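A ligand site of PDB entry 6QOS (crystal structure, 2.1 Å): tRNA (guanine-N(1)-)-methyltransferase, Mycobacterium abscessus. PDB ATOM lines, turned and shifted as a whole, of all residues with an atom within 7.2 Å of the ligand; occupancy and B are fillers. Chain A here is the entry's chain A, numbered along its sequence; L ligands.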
ATOM      1  N   VAL A  84       7.078   6.248  21.180  1.00  0.00           N
ATOM      2  CA  VAL A  84       6.312   6.973  20.159  1.00  0.00           C
ATOM      3  C   VAL A  84       6.903   6.744  18.778  1.00  0.00           C
ATOM      4  O   VAL A  84       7.938   7.316  18.447  1.00  0.00           O
ATOM      5  CB  VAL A  84       6.282   8.490  20.436  1.00  0.00           C
ATOM      6  CG1 VAL A  84       5.311   9.203  19.474  1.00  0.00           C
ATOM      7  CG2 VAL A  84       5.893   8.751  21.890  1.00  0.00           C
ATOM      8  N   PRO A  85       6.272   5.873  17.965  1.00  0.00           N
ATOM      9  CA  PRO A  85       6.770   5.720  16.594  1.00  0.00           C
ATOM     10  C   PRO A  85       6.496   6.956  15.752  1.00  0.00           C
ATOM     11  O   PRO A  85       5.401   7.525  15.775  1.00  0.00           O
ATOM     12  CB  PRO A  85       5.978   4.518  16.046  1.00  0.00           C
ATOM     13  CG  PRO A  85       5.463   3.800  17.316  1.00  0.00           C
ATOM     14  CD  PRO A  85       5.200   4.906  18.288  1.00  0.00           C
ATOM     15  N   THR A  86       7.520   7.357  14.999  1.00  0.00           N
ATOM     16  CA  THR A  86       7.439   8.527  14.128  1.00  0.00           C
ATOM     17  C   THR A  86       8.573   8.468  13.115  1.00  0.00           C
ATOM     18  O   THR A  86       9.670   8.052  13.454  1.00  0.00           O
ATOM     19  CB  THR A  86       7.515   9.861  14.936  1.00  0.00           C
ATOM     20  OG1 THR A  86       7.810  10.931  14.034  1.00  0.00           O
ATOM     21  CG2 THR A  86       8.603   9.802  15.978  1.00  0.00           C
ATOM     22  N   PRO A  87       8.304   8.907  11.877  1.00  0.00           N
ATOM     23  CA  PRO A  87       9.360   9.029  10.856  1.00  0.00           C
ATOM     24  C   PRO A  87      10.495   9.963  11.288  1.00  0.00           C
ATOM     25  O   PRO A  87      11.587   9.862  10.740  1.00  0.00           O
ATOM     26  CB  PRO A  87       8.602   9.610   9.647  1.00  0.00           C
ATOM     27  CG  PRO A  87       7.439  10.302  10.234  1.00  0.00           C
ATOM     28  CD  PRO A  87       7.027   9.484  11.425  1.00  0.00           C
ATOM     29  N   ALA A  88      10.236  10.830  12.264  1.00  0.00           N
ATOM     30  CA  ALA A  88      11.254  11.767  12.737  1.00  0.00           C
ATOM     31  C   ALA A  88      12.042  11.253  13.936  1.00  0.00           C
ATOM     32  O   ALA A  88      12.776  12.008  14.575  1.00  0.00           O
ATOM     33  CB  ALA A  88      10.601  13.108  13.110  1.00  0.00           C
ATOM     34  N   GLY A  89      11.882   9.974  14.254  1.00  0.00           N
ATOM     35  CA  GLY A  89      12.479   9.411  15.448  1.00  0.00           C
ATOM     36  C   GLY A  89      13.948   9.032  15.342  1.00  0.00           C
ATOM     37  O   GLY A  89      14.530   9.038  14.243  1.00  0.00           O
ATOM     38  N   ALA A 109       2.421   4.745  22.037  1.00  0.00           N
ATOM     39  CA  ALA A 109       1.432   5.725  21.577  1.00  0.00           C
ATOM     40  C   ALA A 109       1.405   5.821  20.059  1.00  0.00           C
ATOM     41  O   ALA A 109       2.324   6.396  19.453  1.00  0.00           O
ATOM     42  CB  ALA A 109       1.721   7.086  22.207  1.00  0.00           C
ATOM     43  N   CYS A 110       0.363   5.250  19.444  1.00  0.00           N
ATOM     44  CA  CYS A 110       0.215   5.275  17.976  1.00  0.00           C
ATOM     45  C   CYS A 110      -0.592   6.474  17.484  1.00  0.00           C
ATOM     46  O   CYS A 110      -1.771   6.628  17.846  1.00  0.00           O
ATOM     47  CB  CYS A 110      -0.476   3.994  17.482  1.00  0.00           C
ATOM     48  SG  CYS A 110       0.233   2.446  18.080  1.00  0.00           S
ATOM     49  N   GLY A 111       0.023   7.297  16.649  1.00  0.00           N
ATOM     50  CA  GLY A 111      -0.646   8.432  16.048  1.00  0.00           C
ATOM     51  C   GLY A 111      -0.473   8.476  14.532  1.00  0.00           C
ATOM     52  O   GLY A 111       0.226   7.640  13.950  1.00  0.00           O
ATOM     53  N   ARG A 112      -1.140   9.433  13.895  1.00  0.00           N
ATOM     54  CA  ARG A 112      -1.027   9.616  12.451  1.00  0.00           C
ATOM     55  C   ARG A 112       0.338  10.228  12.132  1.00  0.00           C
ATOM     56  O   ARG A 112       0.962  10.822  13.001  1.00  0.00           O
ATOM     57  CB  ARG A 112      -2.180  10.486  11.913  1.00  0.00           C
ATOM     58  CG  ARG A 112      -2.393  11.820  12.644  1.00  0.00           C
ATOM     59  CD  ARG A 112      -3.650  12.526  12.091  1.00  0.00           C
ATOM     60  NE  ARG A 112      -3.527  12.717  10.641  1.00  0.00           N
ATOM     61  CZ  ARG A 112      -4.528  12.915   9.795  1.00  0.00           C
ATOM     62  NH1 ARG A 112      -5.782  12.955  10.230  1.00  0.00           N
ATOM     63  NH2 ARG A 112      -4.281  13.077   8.507  1.00  0.00           N
ATOM     64  N   TYR A 113       0.801  10.086  10.892  1.00  0.00           N
ATOM     65  CA  TYR A 113       2.202  10.414  10.642  1.00  0.00           C
ATOM     66  C   TYR A 113       2.504  11.913  10.750  1.00  0.00           C
ATOM     67  O   TYR A 113       3.633  12.299  11.064  1.00  0.00           O
ATOM     68  CB  TYR A 113       2.647   9.881   9.273  1.00  0.00           C
ATOM     69  CG  TYR A 113       2.191  10.690   8.100  1.00  0.00           C
ATOM     70  CD1 TYR A 113       0.942  10.478   7.534  1.00  0.00           C
ATOM     71  CD2 TYR A 113       3.020  11.656   7.550  1.00  0.00           C
ATOM     72  CE1 TYR A 113       0.514  11.232   6.438  1.00  0.00           C
ATOM     73  CE2 TYR A 113       2.602  12.415   6.463  1.00  0.00           C
ATOM     74  CZ  TYR A 113       1.349  12.192   5.908  1.00  0.00           C
ATOM     75  OH  TYR A 113       0.951  12.943   4.827  1.00  0.00           O
ATOM     76  N   GLU A 114       1.496  12.754  10.518  1.00  0.00           N
ATOM     77  CA  GLU A 114       1.634  14.211  10.659  1.00  0.00           C
ATOM     78  C   GLU A 114       2.074  14.586  12.069  1.00  0.00           C
ATOM     79  O   GLU A 114       2.720  15.608  12.277  1.00  0.00           O
ATOM     80  CB  GLU A 114       0.330  14.931  10.308  1.00  0.00           C
ATOM     81  CG  GLU A 114      -0.107  14.779   8.849  1.00  0.00           C
ATOM     82  CD  GLU A 114      -0.921  13.525   8.593  1.00  0.00           C
ATOM     83  OE1 GLU A 114      -0.850  12.565   9.390  1.00  0.00           O
ATOM     84  OE2 GLU A 114      -1.651  13.492   7.571  1.00  0.00           O
ATOM     85  N   GLY A 115       1.696  13.759  13.044  1.00  0.00           N
ATOM     86  CA  GLY A 115       2.221  13.878  14.385  1.00  0.00           C
ATOM     87  C   GLY A 115       1.225  14.138  15.505  1.00  0.00           C
ATOM     88  O   GLY A 115       0.055  14.467  15.265  1.00  0.00           O
ATOM     89  N   VAL A 133      10.925   7.052  18.072  1.00  0.00           N
ATOM     90  CA  VAL A 133      11.731   6.166  17.239  1.00  0.00           C
ATOM     91  C   VAL A 133      11.129   5.920  15.862  1.00  0.00           C
ATOM     92  O   VAL A 133       9.913   5.817  15.722  1.00  0.00           O
ATOM     93  CB  VAL A 133      11.963   4.788  17.928  1.00  0.00           C
ATOM     94  CG1 VAL A 133      12.881   4.945  19.146  1.00  0.00           C
ATOM     95  CG2 VAL A 133      10.630   4.110  18.315  1.00  0.00           C
ATOM     96  N   SER A 134      12.004   5.788  14.882  1.00  0.00           N
ATOM     97  CA  SER A 134      11.657   5.373  13.510  1.00  0.00           C
ATOM     98  C   SER A 134      12.091   3.931  13.254  1.00  0.00           C
ATOM     99  O   SER A 134      13.208   3.570  13.602  1.00  0.00           O
ATOM    100  CB  SER A 134      12.333   6.302  12.493  1.00  0.00           C
ATOM    101  OG  SER A 134      12.334   5.760  11.178  1.00  0.00           O
ATOM    102  N   ILE A 135      11.213   3.123  12.668  1.00  0.00           N
ATOM    103  CA  ILE A 135      11.592   1.742  12.363  1.00  0.00           C
ATOM    104  C   ILE A 135      12.131   1.585  10.921  1.00  0.00           C
ATOM    105  O   ILE A 135      12.485   0.481  10.503  1.00  0.00           O
ATOM    106  CB  ILE A 135      10.405   0.741  12.557  1.00  0.00           C
ATOM    107  CG1 ILE A 135       9.231   1.090  11.646  1.00  0.00           C
ATOM    108  CG2 ILE A 135       9.986   0.641  14.045  1.00  0.00           C
ATOM    109  CD1 ILE A 135       8.361  -0.101  11.327  1.00  0.00           C
ATOM    110  N   GLY A 136      12.214   2.694  10.187  1.00  0.00           N
ATOM    111  CA  GLY A 136      12.757   2.663   8.823  1.00  0.00           C
ATOM    112  C   GLY A 136      12.349   3.879   8.011  1.00  0.00           C
ATOM    113  O   GLY A 136      11.426   4.614   8.401  1.00  0.00           O
ATOM    114  N   ASP A 137      13.007   4.081   6.867  1.00  0.00           N
ATOM    115  CA  ASP A 137      12.793   5.290   6.058  1.00  0.00           C
ATOM    116  C   ASP A 137      11.719   5.144   4.982  1.00  0.00           C
ATOM    117  O   ASP A 137      11.989   5.088   3.781  1.00  0.00           O
ATOM    118  CB  ASP A 137      14.108   5.755   5.441  1.00  0.00           C
ATOM    119  CG  ASP A 137      14.997   6.442   6.459  1.00  0.00           C
ATOM    120  OD1 ASP A 137      14.453   7.013   7.438  1.00  0.00           O
ATOM    121  OD2 ASP A 137      16.226   6.406   6.304  1.00  0.00           O
ATOM    122  N   TYR A 138      10.474   5.121   5.449  1.00  0.00           N
ATOM    123  CA  TYR A 138       9.288   5.095   4.606  1.00  0.00           C
ATOM    124  C   TYR A 138       8.177   5.742   5.415  1.00  0.00           C
ATOM    125  O   TYR A 138       8.318   5.955   6.643  1.00  0.00           O
ATOM    126  CB  TYR A 138       8.921   3.656   4.220  1.00  0.00           C
ATOM    127  CG  TYR A 138       9.256   2.648   5.301  1.00  0.00           C
ATOM    128  CD1 TYR A 138       8.486   2.569   6.471  1.00  0.00           C
ATOM    129  CD2 TYR A 138      10.354   1.804   5.176  1.00  0.00           C
ATOM    130  CE1 TYR A 138       8.803   1.644   7.479  1.00  0.00           C
ATOM    131  CE2 TYR A 138      10.671   0.879   6.184  1.00  0.00           C
ATOM    132  CZ  TYR A 138       9.898   0.815   7.335  1.00  0.00           C
ATOM    133  OH  TYR A 138      10.229  -0.090   8.325  1.00  0.00           O
ATOM    134  N   VAL A 139       7.088   6.072   4.740  1.00  0.00           N
ATOM    135  CA  VAL A 139       5.953   6.711   5.390  1.00  0.00           C
ATOM    136  C   VAL A 139       4.775   5.743   5.503  1.00  0.00           C
ATOM    137  O   VAL A 139       4.326   5.172   4.505  1.00  0.00           O
ATOM    138  CB  VAL A 139       5.495   7.971   4.620  1.00  0.00           C
ATOM    139  CG1 VAL A 139       4.335   8.637   5.353  1.00  0.00           C
ATOM    140  CG2 VAL A 139       6.644   8.948   4.450  1.00  0.00           C
ATOM    141  N   LEU A 140       4.292   5.580   6.736  1.00  0.00           N
ATOM    142  CA  LEU A 140       3.017   4.908   7.025  1.00  0.00           C
ATOM    143  C   LEU A 140       1.958   5.958   7.385  1.00  0.00           C
ATOM    144  O   LEU A 140       2.293   7.019   7.902  1.00  0.00           O
ATOM    145  CB  LEU A 140       3.178   3.909   8.176  1.00  0.00           C
ATOM    146  CG  LEU A 140       4.425   3.012   8.102  1.00  0.00           C
ATOM    147  CD1 LEU A 140       4.599   2.164   9.350  1.00  0.00           C
ATOM    148  CD2 LEU A 140       4.347   2.116   6.886  1.00  0.00           C
ATOM    149  N   ASN A 141       0.682   5.658   7.140  1.00  0.00           N
ATOM    150  CA  ASN A 141      -0.379   6.599   7.504  1.00  0.00           C
ATOM    151  C   ASN A 141      -0.458   6.836   9.004  1.00  0.00           C
ATOM    152  O   ASN A 141      -0.872   7.916   9.438  1.00  0.00           O
ATOM    153  CB  ASN A 141      -1.748   6.126   7.022  1.00  0.00           C
ATOM    154  CG  ASN A 141      -2.281   6.986   5.906  1.00  0.00           C
ATOM    155  OD1 ASN A 141      -1.526   7.641   5.188  1.00  0.00           O
ATOM    156  ND2 ASN A 141      -3.609   7.068   5.809  1.00  0.00           N
ATOM    157  N   GLY A 142      -0.054   5.843   9.787  1.00  0.00           N
ATOM    158  CA  GLY A 142      -0.092   5.932  11.242  1.00  0.00           C
ATOM    159  C   GLY A 142       0.895   4.964  11.890  1.00  0.00           C
ATOM    160  O   GLY A 142       1.405   4.071  11.223  1.00  0.00           O
ATOM    161  N   GLY A 143       1.138   5.118  13.181  1.00  0.00           N
ATOM    162  CA  GLY A 143       2.146   4.312  13.848  1.00  0.00           C
ATOM    163  C   GLY A 143       1.793   2.857  14.155  1.00  0.00           C
ATOM    164  O   GLY A 143       2.641   2.123  14.674  1.00  0.00           O
ATOM    165  N   GLU A 144       0.575   2.435  13.806  1.00  0.00           N
ATOM    166  CA  GLU A 144       0.066   1.104  14.166  1.00  0.00           C
ATOM    167  C   GLU A 144       0.960  -0.082  13.702  1.00  0.00           C
ATOM    168  O   GLU A 144       1.318  -0.954  14.504  1.00  0.00           O
ATOM    169  CB  GLU A 144      -1.349   0.931  13.603  1.00  0.00           C
ATOM    170  CG  GLU A 144      -2.476   1.522  14.517  1.00  0.00           C
ATOM    171  CD  GLU A 144      -2.600   3.047  14.442  1.00  0.00           C
ATOM    172  OE1 GLU A 144      -2.108   3.649  13.460  1.00  0.00           O
ATOM    173  OE2 GLU A 144      -3.211   3.652  15.368  1.00  0.00           O
ATOM    174  N   ALA A 146       4.060  -0.012  12.767  1.00  0.00           N
ATOM    175  CA  ALA A 146       5.333   0.147  13.462  1.00  0.00           C
ATOM    176  C   ALA A 146       5.304  -0.408  14.882  1.00  0.00           C
ATOM    177  O   ALA A 146       6.294  -0.992  15.357  1.00  0.00           O
ATOM    178  CB  ALA A 146       5.764   1.614  13.488  1.00  0.00           C
HETATM  179  N1  LIG L   1       9.028   4.569  11.409  1.00  0.00           N
HETATM  180  C1  LIG L   1       8.049   5.276   9.558  1.00  0.00           C
HETATM  181  C2  LIG L   1       7.836   5.083  11.780  1.00  0.00           C
HETATM  182  N2  LIG L   1       9.152   4.688  10.070  1.00  0.00           N
HETATM  183  C3  LIG L   1       3.460   7.595  12.898  1.00  0.00           C
HETATM  184  O1  LIG L   1       5.059   6.360  11.708  1.00  0.00           O
HETATM  185  C4  LIG L   1       3.814   7.016  11.549  1.00  0.00           C
HETATM  186  C5  LIG L   1       5.824   6.194  10.534  1.00  0.00           C
HETATM  187  C6  LIG L   1       7.187   5.539  10.624  1.00  0.00           C
HETATM  188  O2  LIG L   1       5.379   6.564   9.447  1.00  0.00           O
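Pro 85 touches the ligand (O to C3, 3.5 Å). C of Thr 86 touches C2 of the ligand, at 3.7 Å. CD of Pro 87 touches C5 of the ligand, 3.6 Å away. O of Gly 111 touches C3 of the ligand (3.4 Å). Tyr 113 touches the ligand (CA to C3, 3.8 Å). Ser 134 touches the ligand. O of Tyr 138 touches C1 of the ligand, at 3.0 Å. C of Gly 142 touches C4 of the ligand, at 3.6 Å. Gly 143 touches the ligand (N to C3, 3.4 Å). Hydrophobic or aromatic side chains within 4 Å of the ligand: Pro 87, Tyr 113, Ile 135 and Leu 140.
The backbone carbonyl oxygen (O) of Gly 136 sits close to a nitrogen (N2) of the ligand (2.8 Å). The backbone NH (N) of Ile 135 lies close to a nitrogen (N1) of the ligand (2.9 Å). An oxygen (O2) of the ligand is in hydrogen-bond range of the backbone NH of Leu 140 (3.1 Å).
OG of Ser 134 sits at hydrogen-bond distance from O of Gly 136, at 3.1 Å. O of Ile 135 sits at hydrogen-bond distance from OH of Tyr 138, at 3.2 Å. O of Gly 111 sits at hydrogen-bond distance from N of Gly 143, 2.8 Å away. O of Val 133 sits at hydrogen-bond distance from N of Thr 86, 2.9 Å away. The side-chain hydroxyl (OG1) of Thr 86 lies within hydrogen-bond range of the backbone NH (N) of Ala 88 (3.0 Å). The backbone carbonyl oxygen of Asn 141 is in hydrogen-bond range of the backbone NH of Tyr 113 (3.1 Å).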
